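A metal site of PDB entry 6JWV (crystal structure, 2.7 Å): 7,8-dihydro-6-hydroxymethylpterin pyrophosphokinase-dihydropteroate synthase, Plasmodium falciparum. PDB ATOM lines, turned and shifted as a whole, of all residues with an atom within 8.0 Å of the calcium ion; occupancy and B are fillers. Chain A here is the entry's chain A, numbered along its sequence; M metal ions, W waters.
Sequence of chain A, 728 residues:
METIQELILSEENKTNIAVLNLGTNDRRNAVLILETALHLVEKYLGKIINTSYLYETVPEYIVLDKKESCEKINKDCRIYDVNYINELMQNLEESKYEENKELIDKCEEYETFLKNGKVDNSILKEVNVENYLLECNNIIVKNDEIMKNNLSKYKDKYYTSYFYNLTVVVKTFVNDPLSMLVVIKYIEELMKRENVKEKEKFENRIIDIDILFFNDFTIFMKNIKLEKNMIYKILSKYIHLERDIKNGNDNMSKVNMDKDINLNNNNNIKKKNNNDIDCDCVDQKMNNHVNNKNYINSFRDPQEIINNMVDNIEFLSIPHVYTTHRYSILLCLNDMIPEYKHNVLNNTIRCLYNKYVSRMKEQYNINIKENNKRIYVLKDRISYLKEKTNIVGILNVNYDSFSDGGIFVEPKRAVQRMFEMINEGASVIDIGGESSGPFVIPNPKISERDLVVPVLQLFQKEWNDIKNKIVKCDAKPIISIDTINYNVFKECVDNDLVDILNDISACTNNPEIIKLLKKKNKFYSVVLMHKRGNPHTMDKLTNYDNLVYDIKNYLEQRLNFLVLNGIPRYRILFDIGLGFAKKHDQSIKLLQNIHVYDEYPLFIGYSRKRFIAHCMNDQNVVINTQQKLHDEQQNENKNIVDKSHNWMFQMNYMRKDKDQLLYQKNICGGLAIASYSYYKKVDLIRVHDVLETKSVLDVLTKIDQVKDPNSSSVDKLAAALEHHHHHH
Three residues have an atom within 4 Å of the calcium ion: Glu 42, Gly 46 and Glu 99.
OE1 of Glu 99 is bound to the calcium ion (2.2 Å). The backbone carbonyl oxygen (O) of Glu 42 is bound to the calcium ion, 2.3 Å away. O of Gly 46 is bound to the calcium ion (2.5 Å). The calcium ion is bound by water W1, at 2.5 Å. The side-chain carboxylate (OE2) of Glu 42 is bound to the calcium ion, 2.5 Å away. The calcium ion is bound by water W2, at 2.7 Å. OE2 of Glu 99 binds the calcium ion (2.8 Å). The calcium ion has seven donor atoms within binding distance.
The backbone NH of Ile 48 is in hydrogen-bond range of the side-chain carboxylate of Glu 42 (3.2 Å). The side-chain carboxylate of Glu 42 is in salt-bridge range of the side-chain amino group of Lys 518, 3.8 Å away.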
ATOM      1  N   LEU A  38     -37.124   0.657 -30.282  1.00  0.00           N
ATOM      2  CA  LEU A  38     -36.784  -0.440 -29.400  1.00  0.00           C
ATOM      3  C   LEU A  38     -35.648  -1.303 -29.910  1.00  0.00           C
ATOM      4  O   LEU A  38     -34.788  -1.687 -29.106  1.00  0.00           O
ATOM      5  CB  LEU A  38     -37.990  -1.306 -29.060  1.00  0.00           C
ATOM      6  CG  LEU A  38     -39.037  -0.720 -28.096  1.00  0.00           C
ATOM      7  CD1 LEU A  38     -40.111  -1.762 -27.780  1.00  0.00           C
ATOM      8  CD2 LEU A  38     -38.403  -0.223 -26.814  1.00  0.00           C
ATOM      9  N   HIS A  39     -35.614  -1.580 -31.221  1.00  0.00           N
ATOM     10  CA  HIS A  39     -34.556  -2.410 -31.798  1.00  0.00           C
ATOM     11  C   HIS A  39     -33.226  -1.710 -31.674  1.00  0.00           C
ATOM     12  O   HIS A  39     -32.248  -2.311 -31.236  1.00  0.00           O
ATOM     13  CB  HIS A  39     -34.789  -2.743 -33.278  1.00  0.00           C
ATOM     14  CG  HIS A  39     -36.010  -3.564 -33.520  1.00  0.00           C
ATOM     15  ND1 HIS A  39     -36.219  -4.796 -32.941  1.00  0.00           N
ATOM     16  CD2 HIS A  39     -37.082  -3.343 -34.325  1.00  0.00           C
ATOM     17  CE1 HIS A  39     -37.375  -5.283 -33.355  1.00  0.00           C
ATOM     18  NE2 HIS A  39     -37.928  -4.407 -34.171  1.00  0.00           N
ATOM     19  N   LEU A  40     -33.205  -0.433 -32.048  1.00  0.00           N
ATOM     20  CA  LEU A  40     -31.992   0.341 -32.081  1.00  0.00           C
ATOM     21  C   LEU A  40     -31.487   0.601 -30.680  1.00  0.00           C
ATOM     22  O   LEU A  40     -30.272   0.629 -30.475  1.00  0.00           O
ATOM     23  CB  LEU A  40     -32.199   1.641 -32.878  1.00  0.00           C
ATOM     24  CG  LEU A  40     -32.580   1.445 -34.364  1.00  0.00           C
ATOM     25  CD1 LEU A  40     -33.076   2.729 -35.024  1.00  0.00           C
ATOM     26  CD2 LEU A  40     -31.420   0.856 -35.167  1.00  0.00           C
ATOM     27  N   VAL A  41     -32.407   0.749 -29.710  1.00  0.00           N
ATOM     28  CA  VAL A  41     -32.036   0.730 -28.276  1.00  0.00           C
ATOM     29  C   VAL A  41     -31.324  -0.580 -27.924  1.00  0.00           C
ATOM     30  O   VAL A  41     -30.206  -0.577 -27.414  1.00  0.00           O
ATOM     31  CB  VAL A  41     -33.275   0.946 -27.346  1.00  0.00           C
ATOM     32  CG1 VAL A  41     -32.979   0.513 -25.912  1.00  0.00           C
ATOM     33  CG2 VAL A  41     -33.724   2.409 -27.360  1.00  0.00           C
ATOM     34  N   GLU A  42     -31.977  -1.703 -28.227  1.00  0.00           N
ATOM     35  CA  GLU A  42     -31.469  -3.050 -27.930  1.00  0.00           C
ATOM     36  C   GLU A  42     -30.124  -3.308 -28.657  1.00  0.00           C
ATOM     37  O   GLU A  42     -29.270  -4.055 -28.166  1.00  0.00           O
ATOM     38  CB  GLU A  42     -32.551  -4.084 -28.316  1.00  0.00           C
ATOM     39  CG  GLU A  42     -32.240  -5.548 -28.084  1.00  0.00           C
ATOM     40  CD  GLU A  42     -32.128  -5.944 -26.610  1.00  0.00           C
ATOM     41  OE1 GLU A  42     -33.163  -5.939 -25.905  1.00  0.00           O
ATOM     42  OE2 GLU A  42     -30.997  -6.287 -26.186  1.00  0.00           O
ATOM     43  N   LYS A  43     -29.938  -2.666 -29.797  1.00  0.00           N
ATOM     44  CA  LYS A  43     -28.770  -2.889 -30.641  1.00  0.00           C
ATOM     45  C   LYS A  43     -27.591  -2.009 -30.215  1.00  0.00           C
ATOM     46  O   LYS A  43     -26.489  -2.524 -30.072  1.00  0.00           O
ATOM     47  CB  LYS A  43     -29.119  -2.670 -32.121  1.00  0.00           C
ATOM     48  CG  LYS A  43     -27.997  -2.934 -33.110  1.00  0.00           C
ATOM     49  CD  LYS A  43     -28.395  -2.416 -34.481  1.00  0.00           C
ATOM     50  CE  LYS A  43     -27.358  -2.768 -35.527  1.00  0.00           C
ATOM     51  NZ  LYS A  43     -27.172  -4.241 -35.689  1.00  0.00           N
ATOM     52  N   TYR A  44     -27.857  -0.710 -30.013  1.00  0.00           N
ATOM     53  CA  TYR A  44     -26.818   0.276 -29.756  1.00  0.00           C
ATOM     54  C   TYR A  44     -26.564   0.653 -28.302  1.00  0.00           C
ATOM     55  O   TYR A  44     -25.555   1.295 -28.011  1.00  0.00           O
ATOM     56  CB  TYR A  44     -27.072   1.548 -30.590  1.00  0.00           C
ATOM     57  CG  TYR A  44     -26.913   1.369 -32.090  1.00  0.00           C
ATOM     58  CD1 TYR A  44     -25.858   0.622 -32.620  1.00  0.00           C
ATOM     59  CD2 TYR A  44     -27.802   1.978 -32.987  1.00  0.00           C
ATOM     60  CE1 TYR A  44     -25.708   0.451 -33.991  1.00  0.00           C
ATOM     61  CE2 TYR A  44     -27.659   1.813 -34.360  1.00  0.00           C
ATOM     62  CZ  TYR A  44     -26.612   1.050 -34.862  1.00  0.00           C
ATOM     63  OH  TYR A  44     -26.444   0.871 -36.223  1.00  0.00           O
ATOM     64  N   LEU A  45     -27.440   0.264 -27.377  1.00  0.00           N
ATOM     65  CA  LEU A  45     -27.342   0.797 -26.004  1.00  0.00           C
ATOM     66  C   LEU A  45     -27.223  -0.238 -24.888  1.00  0.00           C
ATOM     67  O   LEU A  45     -26.674   0.072 -23.826  1.00  0.00           O
ATOM     68  CB  LEU A  45     -28.504   1.756 -25.706  1.00  0.00           C
ATOM     69  CG  LEU A  45     -28.672   3.027 -26.551  1.00  0.00           C
ATOM     70  CD1 LEU A  45     -30.047   3.636 -26.356  1.00  0.00           C
ATOM     71  CD2 LEU A  45     -27.602   4.016 -26.180  1.00  0.00           C
ATOM     72  N   GLY A  46     -27.697  -1.461 -25.107  1.00  0.00           N
ATOM     73  CA  GLY A  46     -27.699  -2.474 -24.045  1.00  0.00           C
ATOM     74  C   GLY A  46     -28.860  -3.448 -24.154  1.00  0.00           C
ATOM     75  O   GLY A  46     -29.270  -3.812 -25.250  1.00  0.00           O
ATOM     76  N   LYS A  47     -29.382  -3.850 -22.997  1.00  0.00           N
ATOM     77  CA  LYS A  47     -30.438  -4.844 -22.917  1.00  0.00           C
ATOM     78  C   LYS A  47     -31.735  -4.243 -22.373  1.00  0.00           C
ATOM     79  O   LYS A  47     -31.719  -3.596 -21.317  1.00  0.00           O
ATOM     80  CB  LYS A  47     -29.990  -6.020 -22.039  1.00  0.00           C
ATOM     81  CG  LYS A  47     -30.948  -7.197 -22.106  1.00  0.00           C
ATOM     82  CD  LYS A  47     -30.498  -8.427 -21.334  1.00  0.00           C
ATOM     83  CE  LYS A  47     -31.538  -9.541 -21.449  1.00  0.00           C
ATOM     84  NZ  LYS A  47     -31.850  -9.927 -22.871  1.00  0.00           N
ATOM     85  N   ILE A  48     -32.834  -4.437 -23.082  1.00  0.00           N
ATOM     86  CA  ILE A  48     -34.142  -4.011 -22.607  1.00  0.00           C
ATOM     87  C   ILE A  48     -34.618  -5.003 -21.535  1.00  0.00           C
ATOM     88  O   ILE A  48     -34.816  -6.190 -21.821  1.00  0.00           O
ATOM     89  CB  ILE A  48     -35.162  -3.864 -23.745  1.00  0.00           C
ATOM     90  CG1 ILE A  48     -34.725  -2.713 -24.665  1.00  0.00           C
ATOM     91  CG2 ILE A  48     -36.573  -3.644 -23.197  1.00  0.00           C
ATOM     92  CD1 ILE A  48     -35.575  -2.515 -25.901  1.00  0.00           C
ATOM     93  N   SER A  95     -22.878  -2.851 -33.900  1.00  0.00           N
ATOM     94  CA  SER A  95     -22.514  -2.373 -32.565  1.00  0.00           C
ATOM     95  C   SER A  95     -21.187  -2.995 -32.199  1.00  0.00           C
ATOM     96  O   SER A  95     -20.920  -4.143 -32.572  1.00  0.00           O
ATOM     97  CB  SER A  95     -23.572  -2.782 -31.546  1.00  0.00           C
ATOM     98  OG  SER A  95     -23.057  -2.705 -30.215  1.00  0.00           O
ATOM     99  N   TYR A  97     -20.552  -3.757 -29.268  1.00  0.00           N
ATOM    100  CA  TYR A  97     -20.924  -4.588 -28.108  1.00  0.00           C
ATOM    101  C   TYR A  97     -21.875  -5.693 -28.501  1.00  0.00           C
ATOM    102  O   TYR A  97     -22.788  -5.494 -29.294  1.00  0.00           O
ATOM    103  CB  TYR A  97     -21.545  -3.729 -27.002  1.00  0.00           C
ATOM    104  CG  TYR A  97     -20.576  -2.776 -26.354  1.00  0.00           C
ATOM    105  CD1 TYR A  97     -20.143  -1.629 -27.036  1.00  0.00           C
ATOM    106  CD2 TYR A  97     -20.076  -3.018 -25.066  1.00  0.00           C
ATOM    107  CE1 TYR A  97     -19.225  -0.763 -26.461  1.00  0.00           C
ATOM    108  CE2 TYR A  97     -19.169  -2.133 -24.486  1.00  0.00           C
ATOM    109  CZ  TYR A  97     -18.755  -1.013 -25.193  1.00  0.00           C
ATOM    110  OH  TYR A  97     -17.866  -0.125 -24.646  1.00  0.00           O
ATOM    111  N   GLU A  98     -21.660  -6.862 -27.917  1.00  0.00           N
ATOM    112  CA  GLU A  98     -22.374  -8.053 -28.352  1.00  0.00           C
ATOM    113  C   GLU A  98     -23.826  -8.079 -27.911  1.00  0.00           C
ATOM    114  O   GLU A  98     -24.199  -7.482 -26.897  1.00  0.00           O
ATOM    115  CB  GLU A  98     -21.647  -9.318 -27.883  1.00  0.00           C
ATOM    116  CG  GLU A  98     -21.815  -9.611 -26.412  1.00  0.00           C
ATOM    117  CD  GLU A  98     -20.494  -9.681 -25.692  1.00  0.00           C
ATOM    118  OE1 GLU A  98     -19.483 -10.008 -26.354  1.00  0.00           O
ATOM    119  OE2 GLU A  98     -20.468  -9.407 -24.468  1.00  0.00           O
ATOM    120  N   GLU A  99     -24.633  -8.793 -28.693  1.00  0.00           N
ATOM    121  CA  GLU A  99     -26.005  -9.093 -28.328  1.00  0.00           C
ATOM    122  C   GLU A  99     -25.994 -10.460 -27.684  1.00  0.00           C
ATOM    123  O   GLU A  99     -25.345 -11.388 -28.183  1.00  0.00           O
ATOM    124  CB  GLU A  99     -26.882  -9.101 -29.576  1.00  0.00           C
ATOM    125  CG  GLU A  99     -28.382  -9.033 -29.322  1.00  0.00           C
ATOM    126  CD  GLU A  99     -28.796  -7.775 -28.600  1.00  0.00           C
ATOM    127  OE1 GLU A  99     -28.713  -7.742 -27.349  1.00  0.00           O
ATOM    128  OE2 GLU A  99     -29.224  -6.804 -29.264  1.00  0.00           O
ATOM    129  N   ASN A 100     -26.672 -10.578 -26.555  1.00  0.00           N
ATOM    130  CA  ASN A 100     -26.786 -11.851 -25.897  1.00  0.00           C
ATOM    131  C   ASN A 100     -28.243 -12.135 -25.701  1.00  0.00           C
ATOM    132  O   ASN A 100     -28.900 -11.465 -24.913  1.00  0.00           O
ATOM    133  CB  ASN A 100     -26.030 -11.849 -24.579  1.00  0.00           C
ATOM    134  CG  ASN A 100     -24.526 -11.823 -24.771  1.00  0.00           C
ATOM    135  OD1 ASN A 100     -23.972 -12.578 -25.584  1.00  0.00           O
ATOM    136  ND2 ASN A 100     -23.855 -10.950 -24.015  1.00  0.00           N
ATOM    137  N   LYS A 101     -28.750 -13.112 -26.441  1.00  0.00           N
ATOM    138  CA  LYS A 101     -30.153 -13.451 -26.398  1.00  0.00           C
ATOM    139  C   LYS A 101     -30.497 -14.479 -25.319  1.00  0.00           C
ATOM    140  O   LYS A 101     -31.653 -14.769 -25.119  1.00  0.00           O
ATOM    141  CB  LYS A 101     -30.667 -13.890 -27.773  1.00  0.00           C
ATOM    142  CG  LYS A 101     -30.930 -12.711 -28.707  1.00  0.00           C
ATOM    143  CD  LYS A 101     -31.028 -13.081 -30.194  1.00  0.00           C
ATOM    144  CE  LYS A 101     -32.365 -13.717 -30.567  1.00  0.00           C
ATOM    145  NZ  LYS A 101     -33.568 -12.892 -30.222  1.00  0.00           N
ATOM    146  N   VAL A 170     -33.274   0.115 -19.747  1.00  0.00           N
ATOM    147  CA  VAL A 170     -32.148  -0.492 -20.419  1.00  0.00           C
ATOM    148  C   VAL A 170     -31.041  -0.710 -19.398  1.00  0.00           C
ATOM    149  O   VAL A 170     -30.654   0.220 -18.702  1.00  0.00           O
ATOM    150  CB  VAL A 170     -31.598   0.385 -21.559  1.00  0.00           C
ATOM    151  CG1 VAL A 170     -30.827  -0.454 -22.562  1.00  0.00           C
ATOM    152  CG2 VAL A 170     -32.718   1.138 -22.263  1.00  0.00           C
ATOM    153  N   LYS A 171     -30.571  -1.942 -19.308  1.00  0.00           N
ATOM    154  CA  LYS A 171     -29.280  -2.201 -18.688  1.00  0.00           C
ATOM    155  C   LYS A 171     -28.249  -1.835 -19.768  1.00  0.00           C
ATOM    156  O   LYS A 171     -28.107  -2.538 -20.775  1.00  0.00           O
ATOM    157  CB  LYS A 171     -29.186  -3.668 -18.204  1.00  0.00           C
ATOM    158  CG  LYS A 171     -27.781  -4.185 -17.919  1.00  0.00           C
ATOM    159  CD  LYS A 171     -27.747  -5.360 -16.953  1.00  0.00           C
ATOM    160  CE  LYS A 171     -28.269  -6.655 -17.555  1.00  0.00           C
ATOM    161  NZ  LYS A 171     -28.402  -7.725 -16.525  1.00  0.00           N
ATOM    162  N   PHE A 173     -24.451  -0.376 -21.456  1.00  0.00           N
ATOM    163  CA  PHE A 173     -22.976  -0.444 -21.426  1.00  0.00           C
ATOM    164  C   PHE A 173     -22.342   0.923 -21.714  1.00  0.00           C
ATOM    165  O   PHE A 173     -21.126   1.072 -21.673  1.00  0.00           O
ATOM    166  CB  PHE A 173     -22.444  -1.488 -22.428  1.00  0.00           C
ATOM    167  CG  PHE A 173     -23.130  -1.453 -23.776  1.00  0.00           C
ATOM    168  CD1 PHE A 173     -23.058  -0.321 -24.589  1.00  0.00           C
ATOM    169  CD2 PHE A 173     -23.849  -2.562 -24.215  1.00  0.00           C
ATOM    170  CE1 PHE A 173     -23.709  -0.279 -25.814  1.00  0.00           C
ATOM    171  CE2 PHE A 173     -24.496  -2.533 -25.446  1.00  0.00           C
ATOM    172  CZ  PHE A 173     -24.421  -1.394 -26.252  1.00  0.00           C
ATOM    173  N   LYS A 518     -38.721 -12.310 -30.676  1.00  0.00           N
ATOM    174  CA  LYS A 518     -37.995 -11.133 -31.169  1.00  0.00           C
ATOM    175  C   LYS A 518     -37.183 -11.513 -32.384  1.00  0.00           C
ATOM    176  O   LYS A 518     -36.374 -12.431 -32.337  1.00  0.00           O
ATOM    177  CB  LYS A 518     -37.038 -10.572 -30.098  1.00  0.00           C
ATOM    178  CG  LYS A 518     -37.639 -10.396 -28.704  1.00  0.00           C
ATOM    179  CD  LYS A 518     -36.590 -10.536 -27.596  1.00  0.00           C
ATOM    180  CE  LYS A 518     -35.892  -9.215 -27.335  1.00  0.00           C
ATOM    181  NZ  LYS A 518     -35.109  -9.211 -26.069  1.00  0.00           N
HETATM  182 CA    CA M   1     -28.597  -5.667 -26.743  1.00  0.00          CA
HETATM  183  O   HOH W   1     -27.729  -6.420 -24.516  1.00  0.00           O
HETATM  184  O   HOH W   2     -26.073  -5.522 -27.719  1.00  0.00           O
